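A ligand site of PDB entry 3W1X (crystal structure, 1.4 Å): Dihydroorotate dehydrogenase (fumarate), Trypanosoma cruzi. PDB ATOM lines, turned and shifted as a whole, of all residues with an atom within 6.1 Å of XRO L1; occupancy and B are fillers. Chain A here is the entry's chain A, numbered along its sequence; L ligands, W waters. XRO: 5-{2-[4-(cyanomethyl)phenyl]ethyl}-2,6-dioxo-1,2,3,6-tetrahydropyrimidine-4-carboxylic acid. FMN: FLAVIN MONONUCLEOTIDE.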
ATOM      1  N   ALA A  20      12.063  15.733 -15.256  1.00  0.00           N
ATOM      2  CA  ALA A  20      12.407  14.936 -14.116  1.00  0.00           C
ATOM      3  C   ALA A  20      12.429  15.811 -12.884  1.00  0.00           C
ATOM      4  O   ALA A  20      12.876  16.956 -12.871  1.00  0.00           O
ATOM      5  CB  ALA A  20      13.799  14.246 -14.299  1.00  0.00           C
ATOM      6  N   LYS A  44      11.398  10.629 -10.957  1.00  0.00           N
ATOM      7  CA  LYS A  44      12.319  11.442 -10.250  1.00  0.00           C
ATOM      8  C   LYS A  44      13.722  10.805 -10.292  1.00  0.00           C
ATOM      9  O   LYS A  44      13.815   9.616 -10.007  1.00  0.00           O
ATOM     10  CB  LYS A  44      11.856  11.521  -8.758  1.00  0.00           C
ATOM     11  CG  LYS A  44      12.867  12.181  -7.838  1.00  0.00           C
ATOM     12  CD  LYS A  44      13.216  13.721  -7.985  1.00  0.00           C
ATOM     13  CE  LYS A  44      14.494  14.283  -7.269  1.00  0.00           C
ATOM     14  NZ  LYS A  44      14.930  15.844  -7.354  1.00  0.00           N
ATOM     15  N   SER A  45      14.724  11.644 -10.472  1.00  0.00           N
ATOM     16  CA  SER A  45      16.116  11.103 -10.439  1.00  0.00           C
ATOM     17  C   SER A  45      16.335  10.422  -9.103  1.00  0.00           C
ATOM     18  O   SER A  45      16.025  10.944  -8.062  1.00  0.00           O
ATOM     19  CB  SER A  45      17.103  12.191 -10.517  1.00  0.00           C
ATOM     20  OG  SER A  45      17.100  12.769 -11.850  1.00  0.00           O
ATOM     21  N   ASN A  54      17.075  18.011   1.100  1.00  0.00           N
ATOM     22  CA  ASN A  54      17.419  19.153   1.890  1.00  0.00           C
ATOM     23  C   ASN A  54      16.244  19.666   2.699  1.00  0.00           C
ATOM     24  O   ASN A  54      15.140  19.390   2.483  1.00  0.00           O
ATOM     25  CB  ASN A  54      17.967  20.294   0.990  1.00  0.00           C
ATOM     26  CG  ASN A  54      19.345  20.028   0.476  1.00  0.00           C
ATOM     27  OD1 ASN A  54      20.116  19.342   1.067  1.00  0.00           O
ATOM     28  ND2 ASN A  54      19.643  20.592  -0.647  1.00  0.00           N
ATOM     29  N   ASN A  68      15.269  26.127  -6.976  1.00  0.00           N
ATOM     30  CA  ASN A  68      15.237  24.926  -6.164  1.00  0.00           C
ATOM     31  C   ASN A  68      16.624  24.455  -5.747  1.00  0.00           C
ATOM     32  O   ASN A  68      17.564  24.425  -6.527  1.00  0.00           O
ATOM     33  CB  ASN A  68      14.458  23.739  -6.807  1.00  0.00           C
ATOM     34  CG  ASN A  68      15.309  22.891  -7.689  1.00  0.00           C
ATOM     35  OD1 ASN A  68      16.044  21.964  -7.199  1.00  0.00           O
ATOM     36  ND2 ASN A  68      15.269  23.136  -8.973  1.00  0.00           N
ATOM     37  N   SER A  69      16.729  23.996  -4.519  1.00  0.00           N
ATOM     38  CA  SER A  69      17.863  23.184  -4.026  1.00  0.00           C
ATOM     39  C   SER A  69      17.267  21.983  -3.306  1.00  0.00           C
ATOM     40  O   SER A  69      17.411  21.861  -2.063  1.00  0.00           O
ATOM     41  CB  SER A  69      18.775  24.078  -3.167  1.00  0.00           C
ATOM     42  OG  SER A  69      19.516  24.906  -4.011  1.00  0.00           O
ATOM     43  N   MET A  70      16.631  21.092  -4.036  1.00  0.00           N
ATOM     44  CA  MET A  70      15.914  19.958  -3.443  1.00  0.00           C
ATOM     45  C   MET A  70      16.828  18.994  -2.721  1.00  0.00           C
ATOM     46  O   MET A  70      16.495  18.449  -1.656  1.00  0.00           O
ATOM     47  CB  MET A  70      15.141  19.209  -4.487  1.00  0.00           C
ATOM     48  CG  MET A  70      14.150  19.941  -5.293  1.00  0.00           C
ATOM     49  SD  MET A  70      12.884  20.826  -4.321  1.00  0.00           S
ATOM     50  CE  MET A  70      11.895  19.513  -3.814  1.00  0.00           C
ATOM     51  N   GLY A  71      18.001  18.718  -3.288  1.00  0.00           N
ATOM     52  CA  GLY A  71      18.960  17.773  -2.697  1.00  0.00           C
ATOM     53  C   GLY A  71      18.650  16.372  -2.995  1.00  0.00           C
ATOM     54  O   GLY A  71      18.905  15.448  -2.191  1.00  0.00           O
ATOM     55  N   LEU A  72      18.051  16.079  -4.131  1.00  0.00           N
ATOM     56  CA  LEU A  72      17.775  14.720  -4.585  1.00  0.00           C
ATOM     57  C   LEU A  72      16.912  13.944  -3.604  1.00  0.00           C
ATOM     58  O   LEU A  72      17.213  12.772  -3.333  1.00  0.00           O
ATOM     59  CB  LEU A  72      19.068  13.937  -4.886  1.00  0.00           C
ATOM     60  CG  LEU A  72      19.454  13.750  -6.248  1.00  0.00           C
ATOM     61  CD1 LEU A  72      20.827  13.117  -6.332  1.00  0.00           C
ATOM     62  CD2 LEU A  72      18.433  13.113  -7.157  1.00  0.00           C
ATOM     63  N   PRO A  73      15.832  14.437  -3.088  1.00  0.00           N
ATOM     64  CA  PRO A  73      14.912  13.603  -2.322  1.00  0.00           C
ATOM     65  C   PRO A  73      14.283  12.582  -3.243  1.00  0.00           C
ATOM     66  O   PRO A  73      13.894  12.915  -4.365  1.00  0.00           O
ATOM     67  CB  PRO A  73      13.854  14.562  -1.794  1.00  0.00           C
ATOM     68  CG  PRO A  73      13.849  15.680  -2.759  1.00  0.00           C
ATOM     69  CD  PRO A  73      15.246  15.799  -3.404  1.00  0.00           C
ATOM     70  N   SER A 100      20.427   9.320 -10.986  1.00  0.00           N
ATOM     71  CA  SER A 100      21.373  10.360 -10.652  1.00  0.00           C
ATOM     72  C   SER A 100      22.221   9.922  -9.481  1.00  0.00           C
ATOM     73  O   SER A 100      22.263  10.557  -8.404  1.00  0.00           O
ATOM     74  CB  SER A 100      20.551  11.618 -10.406  1.00  0.00           C
ATOM     75  OG  SER A 100      21.417  12.655  -9.978  1.00  0.00           O
ATOM     76  N   LEU A 102      25.441   9.433  -7.096  1.00  0.00           N
ATOM     77  CA  LEU A 102      26.371  10.401  -6.522  1.00  0.00           C
ATOM     78  C   LEU A 102      27.842  10.084  -6.801  1.00  0.00           C
ATOM     79  O   LEU A 102      28.742  10.844  -6.414  1.00  0.00           O
ATOM     80  CB  LEU A 102      26.032  10.620  -5.069  1.00  0.00           C
ATOM     81  CG  LEU A 102      24.656  11.479  -4.987  1.00  0.00           C
ATOM     82  CD1 LEU A 102      24.351  11.561  -3.531  1.00  0.00           C
ATOM     83  CD2 LEU A 102      24.643  12.896  -5.498  1.00  0.00           C
ATOM     84  N   ASN A 128      21.164  11.412 -15.503  1.00  0.00           N
ATOM     85  CA  ASN A 128      21.365  12.796 -15.128  1.00  0.00           C
ATOM     86  C   ASN A 128      22.833  13.139 -14.876  1.00  0.00           C
ATOM     87  O   ASN A 128      23.392  12.739 -13.957  1.00  0.00           O
ATOM     88  CB  ASN A 128      20.565  13.090 -13.848  1.00  0.00           C
ATOM     89  CG  ASN A 128      20.557  14.571 -13.454  1.00  0.00           C
ATOM     90  OD1 ASN A 128      20.993  15.367 -14.143  1.00  0.00           O
ATOM     91  ND2 ASN A 128      20.004  14.842 -12.342  1.00  0.00           N
ATOM     92  N   SER A 130      23.876  16.372 -14.778  1.00  0.00           N
ATOM     93  CA  SER A 130      23.818  17.708 -14.184  1.00  0.00           C
ATOM     94  C   SER A 130      23.596  17.498 -12.777  1.00  0.00           C
ATOM     95  O   SER A 130      22.560  17.736 -12.263  1.00  0.00           O
ATOM     96  CB  SER A 130      22.748  18.604 -14.800  1.00  0.00           C
ATOM     97  OG  SER A 130      22.015  17.916 -15.881  1.00  0.00           O
ATOM     98  N   CYS A 131      24.589  16.928 -12.162  1.00  0.00           N
ATOM     99  CA  CYS A 131      24.535  16.346 -10.896  1.00  0.00           C
ATOM    100  C   CYS A 131      25.933  16.466 -10.173  1.00  0.00           C
ATOM    101  O   CYS A 131      26.956  16.338 -10.759  1.00  0.00           O
ATOM    102  CB  CYS A 131      24.389  14.802 -11.157  1.00  0.00           C
ATOM    103  SG  CYS A 131      24.033  13.827  -9.655  1.00  0.00           S
ATOM    104  N   PRO A 132      25.872  16.640  -8.785  1.00  0.00           N
ATOM    105  CA  PRO A 132      27.174  16.579  -8.075  1.00  0.00           C
ATOM    106  C   PRO A 132      27.984  15.281  -8.109  1.00  0.00           C
ATOM    107  O   PRO A 132      27.509  14.216  -8.143  1.00  0.00           O
ATOM    108  CB  PRO A 132      26.798  16.908  -6.605  1.00  0.00           C
ATOM    109  CG  PRO A 132      25.415  16.523  -6.465  1.00  0.00           C
ATOM    110  CD  PRO A 132      24.800  17.004  -7.722  1.00  0.00           C
ATOM    111  N   LYS A 165      20.656  13.744 -19.483  1.00  0.00           N
ATOM    112  CA  LYS A 165      20.110  15.051 -19.118  1.00  0.00           C
ATOM    113  C   LYS A 165      21.309  15.969 -18.852  1.00  0.00           C
ATOM    114  O   LYS A 165      22.178  15.656 -18.019  1.00  0.00           O
ATOM    115  CB  LYS A 165      19.358  14.957 -17.821  1.00  0.00           C
ATOM    116  CG  LYS A 165      18.676  16.215 -17.298  1.00  0.00           C
ATOM    117  CD  LYS A 165      17.527  16.751 -18.167  1.00  0.00           C
ATOM    118  CE  LYS A 165      16.774  17.866 -17.449  1.00  0.00           C
ATOM    119  NZ  LYS A 165      15.980  17.424 -16.339  1.00  0.00           N
ATOM    120  N   ASN A 195      18.739  20.990 -17.955  1.00  0.00           N
ATOM    121  CA  ASN A 195      18.564  21.065 -16.501  1.00  0.00           C
ATOM    122  C   ASN A 195      18.520  22.565 -16.071  1.00  0.00           C
ATOM    123  O   ASN A 195      18.620  23.399 -16.872  1.00  0.00           O
ATOM    124  CB  ASN A 195      19.658  20.225 -15.739  1.00  0.00           C
ATOM    125  CG  ASN A 195      19.101  19.564 -14.473  1.00  0.00           C
ATOM    126  OD1 ASN A 195      18.495  20.200 -13.714  1.00  0.00           O
ATOM    127  ND2 ASN A 195      19.318  18.282 -14.325  1.00  0.00           N
ATOM    128  N   SER A 196      18.354  22.771 -14.789  1.00  0.00           N
ATOM    129  CA  SER A 196      18.293  24.143 -14.318  1.00  0.00           C
ATOM    130  C   SER A 196      19.546  24.948 -14.576  1.00  0.00           C
ATOM    131  O   SER A 196      20.599  24.459 -14.635  1.00  0.00           O
ATOM    132  CB  SER A 196      17.995  24.288 -12.825  1.00  0.00           C
ATOM    133  OG  SER A 196      18.236  23.237 -12.073  1.00  0.00           O
ATOM    134  N   PRO A 214      18.403  25.831   1.863  1.00  0.00           N
ATOM    135  CA  PRO A 214      19.709  25.260   1.605  1.00  0.00           C
ATOM    136  C   PRO A 214      20.614  26.274   0.891  1.00  0.00           C
ATOM    137  O   PRO A 214      20.153  27.188   0.200  1.00  0.00           O
ATOM    138  CB  PRO A 214      19.361  24.062   0.712  1.00  0.00           C
ATOM    139  CG  PRO A 214      17.959  23.848   0.920  1.00  0.00           C
ATOM    140  CD  PRO A 214      17.358  25.150   1.124  1.00  0.00           C
ATOM    141  N   LYS A 215      21.934  26.047   0.988  1.00  0.00           N
ATOM    142  CA  LYS A 215      22.940  26.688   0.161  1.00  0.00           C
ATOM    143  C   LYS A 215      22.860  28.194   0.252  1.00  0.00           C
ATOM    144  O   LYS A 215      23.137  28.904  -0.711  1.00  0.00           O
ATOM    145  CB  LYS A 215      22.835  26.211  -1.283  1.00  0.00           C
ATOM    146  CG  LYS A 215      23.188  24.717  -1.478  1.00  0.00           C
ATOM    147  CD  LYS A 215      22.941  24.244  -2.925  1.00  0.00           C
ATOM    148  CE  LYS A 215      23.666  25.125  -3.946  1.00  0.00           C
ATOM    149  NZ  LYS A 215      23.681  24.486  -5.293  1.00  0.00           N
ATOM    150  N   GLY A 220      18.936  26.125  -8.316  1.00  0.00           N
ATOM    151  CA  GLY A 220      18.779  26.097  -9.804  1.00  0.00           C
ATOM    152  C   GLY A 220      17.530  26.762 -10.271  1.00  0.00           C
ATOM    153  O   GLY A 220      16.459  26.627  -9.672  1.00  0.00           O
HETATM  154  OAB XRO L   1      18.187  19.521  -6.232  1.00  0.00           O
HETATM  155  CAP XRO L   1      17.806  18.561  -6.903  1.00  0.00           C
HETATM  156  OAE XRO L   1      17.356  17.447  -6.495  1.00  0.00           O
HETATM  157  CAS XRO L   1      17.917  18.721  -8.443  1.00  0.00           C
HETATM  158  NAN XRO L   1      17.320  19.917  -8.870  1.00  0.00           N
HETATM  159  CAU XRO L   1      17.420  20.339 -10.143  1.00  0.00           C
HETATM  160  OAC XRO L   1      16.917  21.386 -10.533  1.00  0.00           O
HETATM  161  NAO XRO L   1      18.012  19.439 -11.022  1.00  0.00           N
HETATM  162  CAV XRO L   1      18.581  18.181 -10.675  1.00  0.00           C
HETATM  163  OAD XRO L   1      19.086  17.470 -11.578  1.00  0.00           O
HETATM  164  CAT XRO L   1      18.455  17.801  -9.314  1.00  0.00           C
HETATM  165  CAM XRO L   1      19.093  16.572  -8.906  1.00  0.00           C
HETATM  166  CAL XRO L   1      20.660  16.628  -8.944  1.00  0.00           C
HETATM  167  CAR XRO L   1      21.159  17.564  -8.002  1.00  0.00           C
HETATM  168  CAI XRO L   1      21.455  17.228  -6.684  1.00  0.00           C
HETATM  169  CAG XRO L   1      21.852  18.277  -5.742  1.00  0.00           C
HETATM  170  CAQ XRO L   1      21.999  19.570  -6.111  1.00  0.00           C
HETATM  171  CAK XRO L   1      22.427  20.682  -5.185  1.00  0.00           C
HETATM  172  CAF XRO L   1      21.197  20.967  -4.296  1.00  0.00           C
HETATM  173  NAA XRO L   1      20.267  21.174  -3.698  1.00  0.00           N
HETATM  174  CAH XRO L   1      21.810  19.895  -7.465  1.00  0.00           C
HETATM  175  CAJ XRO L   1      21.401  18.893  -8.371  1.00  0.00           C
HETATM  176  N1  FMN L   2      16.152  17.516 -13.172  1.00  0.00           N
HETATM  177  C2  FMN L   2      16.622  16.228 -13.108  1.00  0.00           C
HETATM  178  O2  FMN L   2      17.163  15.795 -14.150  1.00  0.00           O
HETATM  179  N3  FMN L   2      16.424  15.431 -12.054  1.00  0.00           N
HETATM  180  C4  FMN L   2      15.735  15.833 -11.001  1.00  0.00           C
HETATM  181  O4  FMN L   2      15.530  15.040 -10.041  1.00  0.00           O
HETATM  182  C4A FMN L   2      15.261  17.186 -10.933  1.00  0.00           C
HETATM  183  N5  FMN L   2      14.578  17.647  -9.893  1.00  0.00           N
HETATM  184  C5A FMN L   2      13.878  18.847  -9.978  1.00  0.00           C
HETATM  185  C6  FMN L   2      13.061  19.258  -8.946  1.00  0.00           C
HETATM  186  C7  FMN L   2      12.372  20.434  -9.006  1.00  0.00           C
HETATM  187  C7M FMN L   2      11.445  20.920  -7.914  1.00  0.00           C
HETATM  188  C8  FMN L   2      12.531  21.288 -10.170  1.00  0.00           C
HETATM  189  C8M FMN L   2      11.816  22.617 -10.316  1.00  0.00           C
HETATM  190  C9  FMN L   2      13.392  20.875 -11.191  1.00  0.00           C
HETATM  191  C9A FMN L   2      14.072  19.657 -11.122  1.00  0.00           C
HETATM  192  N10 FMN L   2      14.974  19.236 -12.159  1.00  0.00           N
HETATM  193  C10 FMN L   2      15.462  17.962 -12.106  1.00  0.00           C
HETATM  194  C1' FMN L   2      15.135  20.067 -13.384  1.00  0.00           C
HETATM  195  C2' FMN L   2      13.960  20.013 -14.312  1.00  0.00           C
HETATM  196  O2' FMN L   2      13.906  18.655 -14.821  1.00  0.00           O
HETATM  197  C3' FMN L   2      14.185  20.910 -15.468  1.00  0.00           C
HETATM  198  O3' FMN L   2      15.379  20.534 -16.170  1.00  0.00           O
HETATM  199  C4' FMN L   2      14.325  22.400 -15.073  1.00  0.00           C
HETATM  200  O4' FMN L   2      13.355  22.700 -14.042  1.00  0.00           O
HETATM  201  C5' FMN L   2      14.054  23.349 -16.236  1.00  0.00           C
HETATM  202  O5' FMN L   2      12.785  23.178 -16.843  1.00  0.00           O
HETATM  203  P   FMN L   2      11.588  24.233 -16.526  1.00  0.00           P
HETATM  204  O1P FMN L   2      10.387  23.667 -17.269  1.00  0.00           O
HETATM  205  O2P FMN L   2      12.038  25.576 -17.017  1.00  0.00           O
HETATM  206  O3P FMN L   2      11.429  24.229 -14.970  1.00  0.00           O
HETATM  207  O   HOH W   1      22.667  20.361  -1.260  1.00  0.00           O
HETATM  208  O   HOH W   2      19.121  21.978  -7.228  1.00  0.00           O
HETATM  209  O   HOH W   3      20.946  23.839  -6.133  1.00  0.00           O
HETATM  210  O   HOH W   4      25.845  20.203  -5.243  1.00  0.00           O
HETATM  211  O   HOH W   5      19.751  22.278  -9.975  1.00  0.00           O
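The side-chain hydroxyl of Ser 196 lies within hydrogen-bond range of an oxygen (OAC) of XRO L1 (2.7 Å). An oxygen (OAE) of XRO L1 sits at hydrogen-bond distance from the backbone NH (N) of Leu 72. OD1 of Asn 195 sits at hydrogen-bond distance from NAO of XRO L1 (2.8 Å). The side-chain amide nitrogen (ND2) of Asn 68 lies within hydrogen-bond range of an oxygen (OAC) of XRO L1 (2.9 Å). ND2 of Asn 128 lies within hydrogen-bond range of OAD of XRO L1, at 2.9 Å. The side-chain amino group (NZ) of Lys 44 lies within salt-bridge range of an oxygen (OAE) of XRO L1 (3.0 Å). The backbone NH of Gly 71 is in hydrogen-bond range of an oxygen (OAB) of XRO L1, at 3.1 Å. N of Met 70 is in hydrogen-bond range of OAB of XRO L1 (3.1 Å). ND2 of Asn 54 is in hydrogen-bond range of NAA of XRO L1. The side-chain amide nitrogen (ND2) of Asn 195 sits at hydrogen-bond distance from an oxygen (O2) of FMN L2, at 3.3 Å. O4 of FMN L2 lies within hydrogen-bond range of NZ of Lys 44, at 2.9 Å. The side-chain hydroxyl (OG) of Ser 45 lies within hydrogen-bond range of a nitrogen (N3) of FMN L2. An oxygen (O2') of FMN L2 lies within hydrogen-bond range of the side-chain amino group (NZ) of Lys 165 (2.8 Å). The backbone NH (N) of Ala 20 is in hydrogen-bond range of an oxygen (O2') of FMN L2, 3.5 Å away. The backbone carbonyl oxygen (O) of Ala 20 sits at hydrogen-bond distance from an oxygen (O2') of FMN L2 (2.8 Å).
An oxygen (OAD) of XRO L1 lies close to a nitrogen (N3) of FMN L2, at 3.4 Å.
The side-chain hydroxyl (OG) of Ser 196 sits at hydrogen-bond distance from the side-chain amide oxygen (OD1) of Asn 195, at 3.5 Å. OD1 of Asn 128 lies within hydrogen-bond range of ND2 of Asn 195 (3.4 Å). The side-chain amide oxygen of Asn 68 lies within hydrogen-bond range of the backbone NH of Met 70. The backbone NH of Gly 220 lies within hydrogen-bond range of the backbone carbonyl oxygen of Asn 68. The backbone NH of Ser 130 is in hydrogen-bond range of the side-chain amide oxygen of Asn 128 (3.1 Å). The backbone carbonyl oxygen (O) of Met 70 lies within hydrogen-bond range of the backbone NH (N) of Asn 54. The backbone carbonyl oxygen (O) of Ser 69 is in hydrogen-bond range of the side-chain amide nitrogen (ND2) of Asn 54 (2.9 Å). The side-chain hydroxyl (OG) of Ser 130 is in hydrogen-bond range of the backbone carbonyl oxygen (O) of Lys 165 (3.1 Å).
The backbone carbonyl oxygen (O) of Ser 69 lies close to a nitrogen (NAA) of XRO L1 (3.4 Å). Ser 130 touches XRO L1. Pro 132 touches XRO L1 (CD to CAI, 3.5 Å). CD of Lys 215 touches CAF of XRO L1, at 3.96 Å. Hydrophobic or aromatic side chains within 4 Å of XRO L1: Met 70, Leu 72 and Pro 132. Within 4 Å of XRO L1: Lys 44, Asn 54, Asn 68, Ser 69, Met 70, Gly 71, Leu 72, Asn 128, Ser 130, Pro 132, Asn 195, Ser 196 and Lys 215.
Water W2 lies within hydrogen-bond range of an oxygen (OAB) of XRO L1 (2.8 Å) and the backbone carbonyl oxygen of Asn 68 (3.0 Å). Water W5 lies within hydrogen-bond range of the side-chain hydroxyl (OG) of Ser 196 and an oxygen (OAC) of XRO L1. Water W3 lies within hydrogen-bond range of OG of Ser 69 (2.8 Å), NZ of Lys 215 (2.9 Å) and O of Asn 68 (3.5 Å).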
